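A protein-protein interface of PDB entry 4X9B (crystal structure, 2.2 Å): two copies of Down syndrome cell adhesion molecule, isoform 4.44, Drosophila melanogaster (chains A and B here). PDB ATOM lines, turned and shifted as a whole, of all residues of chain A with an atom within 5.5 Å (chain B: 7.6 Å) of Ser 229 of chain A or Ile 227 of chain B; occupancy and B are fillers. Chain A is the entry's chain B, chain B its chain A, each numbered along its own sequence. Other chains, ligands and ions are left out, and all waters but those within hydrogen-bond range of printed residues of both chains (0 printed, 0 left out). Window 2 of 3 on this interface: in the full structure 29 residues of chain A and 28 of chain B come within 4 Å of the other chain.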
ATOM      1  N   SER A 225       1.217 -17.797   7.474  1.00  0.00           N
ATOM      2  CA  SER A 225       1.945 -16.598   7.057  1.00  0.00           C
ATOM      3  C   SER A 225       0.996 -15.475   6.663  1.00  0.00           C
ATOM      4  O   SER A 225       0.106 -15.669   5.841  1.00  0.00           O
ATOM      5  CB  SER A 225       2.870 -16.922   5.887  1.00  0.00           C
ATOM      6  OG  SER A 225       3.557 -15.766   5.449  1.00  0.00           O
ATOM      7  N   ILE A 227       2.108 -12.628   5.299  1.00  0.00           N
ATOM      8  CA  ILE A 227       2.691 -11.863   4.203  1.00  0.00           C
ATOM      9  C   ILE A 227       3.439 -12.748   3.201  1.00  0.00           C
ATOM     10  O   ILE A 227       4.027 -13.767   3.554  1.00  0.00           O
ATOM     11  CB  ILE A 227       3.647 -10.753   4.732  1.00  0.00           C
ATOM     12  CG1 ILE A 227       3.940  -9.743   3.618  1.00  0.00           C
ATOM     13  CG2 ILE A 227       4.939 -11.353   5.298  1.00  0.00           C
ATOM     14  CD1 ILE A 227       4.648  -8.476   4.090  1.00  0.00           C
ATOM     15  N   SER A 228       3.367 -12.356   1.934  1.00  0.00           N
ATOM     16  CA  SER A 228       4.134 -12.985   0.868  1.00  0.00           C
ATOM     17  C   SER A 228       4.502 -11.916  -0.140  1.00  0.00           C
ATOM     18  O   SER A 228       3.993 -10.800  -0.078  1.00  0.00           O
ATOM     19  CB  SER A 228       3.356 -14.115   0.195  1.00  0.00           C
ATOM     20  OG  SER A 228       2.435 -13.611  -0.753  1.00  0.00           O
ATOM     21  N   SER A 229       5.419 -12.241  -1.043  1.00  0.00           N
ATOM     22  CA  SER A 229       5.722 -11.355  -2.157  1.00  0.00           C
ATOM     23  C   SER A 229       5.668 -12.128  -3.451  1.00  0.00           C
ATOM     24  O   SER A 229       5.798 -13.351  -3.462  1.00  0.00           O
ATOM     25  CB  SER A 229       7.103 -10.726  -2.003  1.00  0.00           C
ATOM     26  OG  SER A 229       8.104 -11.707  -2.210  1.00  0.00           O
ATOM     27  N   LEU A 230       5.480 -11.412  -4.549  1.00  0.00           N
ATOM     28  CA  LEU A 230       5.605 -12.027  -5.852  1.00  0.00           C
ATOM     29  C   LEU A 230       6.015 -11.003  -6.890  1.00  0.00           C
ATOM     30  O   LEU A 230       5.797  -9.800  -6.734  1.00  0.00           O
ATOM     31  CB  LEU A 230       4.302 -12.714  -6.254  1.00  0.00           C
ATOM     32  CG  LEU A 230       3.030 -11.885  -6.373  1.00  0.00           C
ATOM     33  CD1 LEU A 230       2.883 -11.311  -7.758  1.00  0.00           C
ATOM     34  CD2 LEU A 230       1.841 -12.773  -6.052  1.00  0.00           C
ATOM     35  N   LEU A 231       6.616 -11.516  -7.951  1.00  0.00           N
ATOM     36  CA  LEU A 231       7.138 -10.707  -9.027  1.00  0.00           C
ATOM     37  C   LEU A 231       6.287 -10.952 -10.268  1.00  0.00           C
ATOM     38  O   LEU A 231       5.746 -12.043 -10.456  1.00  0.00           O
ATOM     39  CB  LEU A 231       8.606 -11.058  -9.273  1.00  0.00           C
ATOM     40  CG  LEU A 231       9.433 -10.097 -10.122  1.00  0.00           C
ATOM     41  CD1 LEU A 231      10.751  -9.826  -9.441  1.00  0.00           C
ATOM     42  CD2 LEU A 231       9.659 -10.679 -11.504  1.00  0.00           C
ATOM     43  N   THR A 308       0.150  -9.084   0.373  1.00  0.00           N
ATOM     44  CA  THR A 308       0.977  -9.536  -0.738  1.00  0.00           C
ATOM     45  C   THR A 308       1.724  -8.342  -1.318  1.00  0.00           C
ATOM     46  O   THR A 308       1.111  -7.338  -1.665  1.00  0.00           O
ATOM     47  CB  THR A 308       0.128 -10.209  -1.833  1.00  0.00           C
ATOM     48  OG1 THR A 308      -0.688 -11.231  -1.246  1.00  0.00           O
ATOM     49  CG2 THR A 308       1.018 -10.819  -2.912  1.00  0.00           C
ATOM     50  N   VAL A 309       3.047  -8.443  -1.400  1.00  0.00           N
ATOM     51  CA  VAL A 309       3.854  -7.380  -1.987  1.00  0.00           C
ATOM     52  C   VAL A 309       4.091  -7.710  -3.451  1.00  0.00           C
ATOM     53  O   VAL A 309       4.781  -8.677  -3.778  1.00  0.00           O
ATOM     54  CB  VAL A 309       5.203  -7.203  -1.252  1.00  0.00           C
ATOM     55  CG1 VAL A 309       6.089  -6.208  -1.980  1.00  0.00           C
ATOM     56  CG2 VAL A 309       4.970  -6.732   0.168  1.00  0.00           C
ATOM     57  N   LEU A 310       3.511  -6.902  -4.331  1.00  0.00           N
ATOM     58  CA  LEU A 310       3.654  -7.116  -5.762  1.00  0.00           C
ATOM     59  C   LEU A 310       4.686  -6.171  -6.349  1.00  0.00           C
ATOM     60  O   LEU A 310       4.602  -4.959  -6.165  1.00  0.00           O
ATOM     61  CB  LEU A 310       2.320  -6.922  -6.470  1.00  0.00           C
ATOM     62  CG  LEU A 310       2.407  -6.817  -7.993  1.00  0.00           C
ATOM     63  CD1 LEU A 310       3.073  -8.044  -8.592  1.00  0.00           C
ATOM     64  CD2 LEU A 310       1.022  -6.632  -8.577  1.00  0.00           C
ATOM     65  N   THR B 223       9.470 -22.026  -2.633  1.00  0.00           N
ATOM     66  CA  THR B 223       8.480 -21.041  -3.056  1.00  0.00           C
ATOM     67  C   THR B 223       9.183 -19.836  -3.669  1.00  0.00           C
ATOM     68  O   THR B 223      10.345 -19.571  -3.375  1.00  0.00           O
ATOM     69  CB  THR B 223       7.595 -20.580  -1.871  1.00  0.00           C
ATOM     70  OG1 THR B 223       6.812 -19.452  -2.269  1.00  0.00           O
ATOM     71  CG2 THR B 223       8.452 -20.189  -0.665  1.00  0.00           C
ATOM     72  N   ALA B 224       8.476 -19.108  -4.526  1.00  0.00           N
ATOM     73  CA  ALA B 224       9.043 -17.932  -5.168  1.00  0.00           C
ATOM     74  C   ALA B 224       8.893 -16.698  -4.286  1.00  0.00           C
ATOM     75  O   ALA B 224       9.409 -15.631  -4.610  1.00  0.00           O
ATOM     76  CB  ALA B 224       8.388 -17.699  -6.505  1.00  0.00           C
ATOM     77  N   SER B 225       8.182 -16.850  -3.175  1.00  0.00           N
ATOM     78  CA  SER B 225       7.977 -15.755  -2.243  1.00  0.00           C
ATOM     79  C   SER B 225       9.285 -15.418  -1.546  1.00  0.00           C
ATOM     80  O   SER B 225      10.010 -16.316  -1.113  1.00  0.00           O
ATOM     81  CB  SER B 225       6.902 -16.121  -1.217  1.00  0.00           C
ATOM     82  OG  SER B 225       6.637 -15.039  -0.334  1.00  0.00           O
ATOM     83  N   LYS B 226       9.601 -14.129  -1.469  1.00  0.00           N
ATOM     84  CA  LYS B 226      10.816 -13.682  -0.792  1.00  0.00           C
ATOM     85  C   LYS B 226      10.564 -13.231   0.643  1.00  0.00           C
ATOM     86  O   LYS B 226      11.488 -12.784   1.319  1.00  0.00           O
ATOM     87  CB  LYS B 226      11.475 -12.558  -1.587  1.00  0.00           C
ATOM     88  CG  LYS B 226      12.062 -13.035  -2.908  1.00  0.00           C
ATOM     89  CD  LYS B 226      12.861 -11.934  -3.583  1.00  0.00           C
ATOM     90  CE  LYS B 226      14.231 -12.414  -4.044  1.00  0.00           C
ATOM     91  NZ  LYS B 226      15.214 -11.297  -4.054  1.00  0.00           N
ATOM     92  N   ILE B 227       9.316 -13.325   1.097  1.00  0.00           N
ATOM     93  CA  ILE B 227       8.958 -12.929   2.461  1.00  0.00           C
ATOM     94  C   ILE B 227       7.817 -13.789   3.015  1.00  0.00           C
ATOM     95  O   ILE B 227       6.886 -14.127   2.299  1.00  0.00           O
ATOM     96  CB  ILE B 227       8.547 -11.424   2.522  1.00  0.00           C
ATOM     97  CG1 ILE B 227       8.205 -10.983   3.946  1.00  0.00           C
ATOM     98  CG2 ILE B 227       7.340 -11.143   1.633  1.00  0.00           C
ATOM     99  CD1 ILE B 227       9.355 -10.926   4.856  1.00  0.00           C
ATOM    100  N   SER B 228       7.900 -14.125   4.295  1.00  0.00           N
ATOM    101  CA  SER B 228       6.821 -14.806   5.002  1.00  0.00           C
ATOM    102  C   SER B 228       6.811 -14.303   6.432  1.00  0.00           C
ATOM    103  O   SER B 228       7.753 -13.639   6.857  1.00  0.00           O
ATOM    104  CB  SER B 228       6.993 -16.325   4.968  1.00  0.00           C
ATOM    105  OG  SER B 228       8.072 -16.721   5.796  1.00  0.00           O
ATOM    106  N   SER B 229       5.747 -14.592   7.175  1.00  0.00           N
ATOM    107  CA  SER B 229       5.705 -14.219   8.584  1.00  0.00           C
ATOM    108  C   SER B 229       5.345 -15.413   9.448  1.00  0.00           C
ATOM    109  O   SER B 229       4.787 -16.408   8.976  1.00  0.00           O
ATOM    110  CB  SER B 229       4.715 -13.073   8.821  1.00  0.00           C
ATOM    111  OG  SER B 229       3.383 -13.480   8.582  1.00  0.00           O
ATOM    112  N   PHE B 257      17.702  -8.317  10.880  1.00  0.00           N
ATOM    113  CA  PHE B 257      17.757  -6.893  10.566  1.00  0.00           C
ATOM    114  C   PHE B 257      17.825  -6.081  11.843  1.00  0.00           C
ATOM    115  O   PHE B 257      17.297  -6.474  12.885  1.00  0.00           O
ATOM    116  CB  PHE B 257      16.561  -6.455   9.722  1.00  0.00           C
ATOM    117  CG  PHE B 257      16.628  -6.925   8.302  1.00  0.00           C
ATOM    118  CD1 PHE B 257      17.360  -6.224   7.362  1.00  0.00           C
ATOM    119  CD2 PHE B 257      15.981  -8.084   7.911  1.00  0.00           C
ATOM    120  CE1 PHE B 257      17.436  -6.661   6.052  1.00  0.00           C
ATOM    121  CE2 PHE B 257      16.051  -8.527   6.607  1.00  0.00           C
ATOM    122  CZ  PHE B 257      16.784  -7.816   5.674  1.00  0.00           C
ATOM    123  N   LYS B 292      12.785  -9.030  12.014  1.00  0.00           N
ATOM    124  CA  LYS B 292      12.899  -9.540  10.657  1.00  0.00           C
ATOM    125  C   LYS B 292      14.219 -10.281  10.486  1.00  0.00           C
ATOM    126  O   LYS B 292      15.296  -9.734  10.726  1.00  0.00           O
ATOM    127  CB  LYS B 292      12.782  -8.418   9.631  1.00  0.00           C
ATOM    128  CG  LYS B 292      12.614  -8.934   8.201  1.00  0.00           C
ATOM    129  CD  LYS B 292      12.731  -7.831   7.164  1.00  0.00           C
ATOM    130  CE  LYS B 292      11.413  -7.121   6.921  1.00  0.00           C
ATOM    131  NZ  LYS B 292      11.485  -6.242   5.717  1.00  0.00           N
ATOM    132  N   TYR B 293      14.103 -11.540  10.077  1.00  0.00           N
ATOM    133  CA  TYR B 293      15.236 -12.431   9.874  1.00  0.00           C
ATOM    134  C   TYR B 293      15.486 -12.596   8.388  1.00  0.00           C
ATOM    135  O   TYR B 293      14.566 -12.469   7.580  1.00  0.00           O
ATOM    136  CB  TYR B 293      14.981 -13.790  10.524  1.00  0.00           C
ATOM    137  CG  TYR B 293      15.073 -13.756  12.023  1.00  0.00           C
ATOM    138  CD1 TYR B 293      13.986 -13.369  12.802  1.00  0.00           C
ATOM    139  CD2 TYR B 293      16.259 -14.092  12.664  1.00  0.00           C
ATOM    140  CE1 TYR B 293      14.081 -13.324  14.187  1.00  0.00           C
ATOM    141  CE2 TYR B 293      16.367 -14.043  14.039  1.00  0.00           C
ATOM    142  CZ  TYR B 293      15.279 -13.661  14.797  1.00  0.00           C
ATOM    143  OH  TYR B 293      15.402 -13.627  16.163  1.00  0.00           O
ATOM    144  N   SER B 305      18.321 -14.940  -1.214  1.00  0.00           N
ATOM    145  CA  SER B 305      17.932 -14.627   0.148  1.00  0.00           C
ATOM    146  C   SER B 305      16.425 -14.490   0.310  1.00  0.00           C
ATOM    147  O   SER B 305      15.714 -14.116  -0.621  1.00  0.00           O
ATOM    148  CB  SER B 305      18.626 -13.345   0.608  1.00  0.00           C
ATOM    149  OG  SER B 305      18.388 -12.298  -0.310  1.00  0.00           O
ATOM    150  N   VAL B 306      15.953 -14.794   1.516  1.00  0.00           N
ATOM    151  CA  VAL B 306      14.538 -14.764   1.830  1.00  0.00           C
ATOM    152  C   VAL B 306      14.346 -14.226   3.235  1.00  0.00           C
ATOM    153  O   VAL B 306      15.136 -14.518   4.133  1.00  0.00           O
ATOM    154  CB  VAL B 306      13.911 -16.170   1.710  1.00  0.00           C
ATOM    155  CG1 VAL B 306      12.469 -16.172   2.204  1.00  0.00           C
ATOM    156  CG2 VAL B 306      13.966 -16.636   0.270  1.00  0.00           C
ATOM    157  N   GLU B 307      13.281 -13.453   3.414  1.00  0.00           N
ATOM    158  CA  GLU B 307      12.970 -12.828   4.690  1.00  0.00           C
ATOM    159  C   GLU B 307      11.865 -13.556   5.456  1.00  0.00           C
ATOM    160  O   GLU B 307      10.910 -14.063   4.860  1.00  0.00           O
ATOM    161  CB  GLU B 307      12.554 -11.379   4.463  1.00  0.00           C
ATOM    162  CG  GLU B 307      13.619 -10.531   3.804  1.00  0.00           C
ATOM    163  CD  GLU B 307      13.255  -9.063   3.773  1.00  0.00           C
ATOM    164  OE1 GLU B 307      12.102  -8.725   4.135  1.00  0.00           O
ATOM    165  OE2 GLU B 307      14.130  -8.254   3.390  1.00  0.00           O
ATOM    166  N   THR B 308      12.002 -13.582   6.780  1.00  0.00           N
ATOM    167  CA  THR B 308      10.962 -14.094   7.676  1.00  0.00           C
ATOM    168  C   THR B 308      10.703 -13.107   8.809  1.00  0.00           C
ATOM    169  O   THR B 308      11.620 -12.755   9.549  1.00  0.00           O
ATOM    170  CB  THR B 308      11.356 -15.450   8.288  1.00  0.00           C
ATOM    171  OG1 THR B 308      11.651 -16.386   7.245  1.00  0.00           O
ATOM    172  CG2 THR B 308      10.239 -15.990   9.159  1.00  0.00           C
ATOM    173  N   VAL B 309       9.462 -12.654   8.942  1.00  0.00           N
ATOM    174  CA  VAL B 309       9.089 -11.753  10.028  1.00  0.00           C
ATOM    175  C   VAL B 309       8.546 -12.569  11.195  1.00  0.00           C
ATOM    176  O   VAL B 309       7.543 -13.271  11.066  1.00  0.00           O
ATOM    177  CB  VAL B 309       8.043 -10.716   9.572  1.00  0.00           C
ATOM    178  CG1 VAL B 309       7.601  -9.837  10.729  1.00  0.00           C
ATOM    179  CG2 VAL B 309       8.611  -9.868   8.477  1.00  0.00           C
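Hydrophobic or aromatic side chains of chain A within 4 Å of the printed part of chain B: Ile 227.
Among the printed residues, 10 pairs touch across the chains.
Among the printed residues, no Asp or Glu carboxylate lies within 4 Å of a Lys or Arg side-chain nitrogen of the other chain.
O of Ser 228 of chain B sits at hydrogen-bond distance from N of Val 309 of chain B.
The side-chain hydroxyl (OG) of Ser 225 of chain A lies within hydrogen-bond range of the backbone carbonyl oxygen (O) of Ile 227 of chain A, at 2.8 Å.
The side-chain hydroxyl (OG) of Ser 225 of chain B is in hydrogen-bond range of the backbone carbonyl oxygen (O) of Ile 227 of chain B, 2.8 Å away.
The backbone carbonyl oxygen (O) of Glu 307 of chain B is in hydrogen-bond range of the backbone NH (N) of Ser 228 of chain B (3.1 Å).
O of Lys 226 of chain B is in hydrogen-bond range of N of Glu 307 of chain B (2.8 Å).
O of Ser 228 of chain A sits at hydrogen-bond distance from N of Val 309 of chain A, 2.9 Å away.
OG of Ser 225 of chain B sits at hydrogen-bond distance from N of Ser 229 of chain A (3.1 Å).
The backbone carbonyl oxygen (O) of Ile 227 of chain B sits close to the backbone carbonyl oxygen (O) of Ile 227 of chain A, at 3.1 Å.
N of Lys 226 of chain B sits at hydrogen-bond distance from OG of Ser 229 of chain A (2.9 Å).
The backbone NH of Ser 229 of chain B sits at hydrogen-bond distance from the side-chain hydroxyl of Ser 225 of chain A.
Ser 225 of chain A touches Ser 228 of chain B, and with the chains exchanged Ser 228 of chain A touches Ser 225 of chain B.
Ser 225 of chain A touches Ser 229 of chain B, and with the chains exchanged Ser 229 of chain A touches Ser 225 of chain B.
Ile 227 of chain A touches its own counterpart, Ile 227 of chain B.
Ile 227 of chain A touches Ser 229 of chain B, and with the chains exchanged Ser 229 of chain A touches Ile 227 of chain B.
6 positions are printed for both chains.
Among the printed residues, merely in contact across the chains: Ser 228 of chain A with Ile 227 of chain B (3.3 Å), Ile 227 of chain A with Ser 228 of chain B (3.3 Å), Ser 225 of chain A with Ser 228 of chain B (3.4 Å), Ser 228 of chain A with Ser 225 of chain B (3.4 Å), Ser 229 of chain A with Ile 227 of chain B (3.5 Å) and Ile 227 of chain A with Ser 229 of chain B (3.6 Å).
Printed residues of chain B within 4 Å of Ser 225 of chain A: Ser 228 and Ser 229.
Of the printed residues of chain B, Ile 227 of chain A touches Ile 227 (3.1 Å), Ser 228 (3.3 Å) and Ser 229 (3.6 Å).
Of the printed residues of chain B, Ser 228 of chain A touches Ser 225 and Ile 227.
Ser 229 of chain A touches just these residues of chain B: Ser 225, Lys 226 and Ile 227.
Ile 227 of chain B touches three residues of chain A.
Printed residues of chain A within 4 Å of Ser 228 of chain B: Ser 225 (3.4 Å) and Ile 227 (3.3 Å).
The nearest printed residue of chain B that does not touch Ile 227 of chain A is Ser 225 of chain B (4.9 Å).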
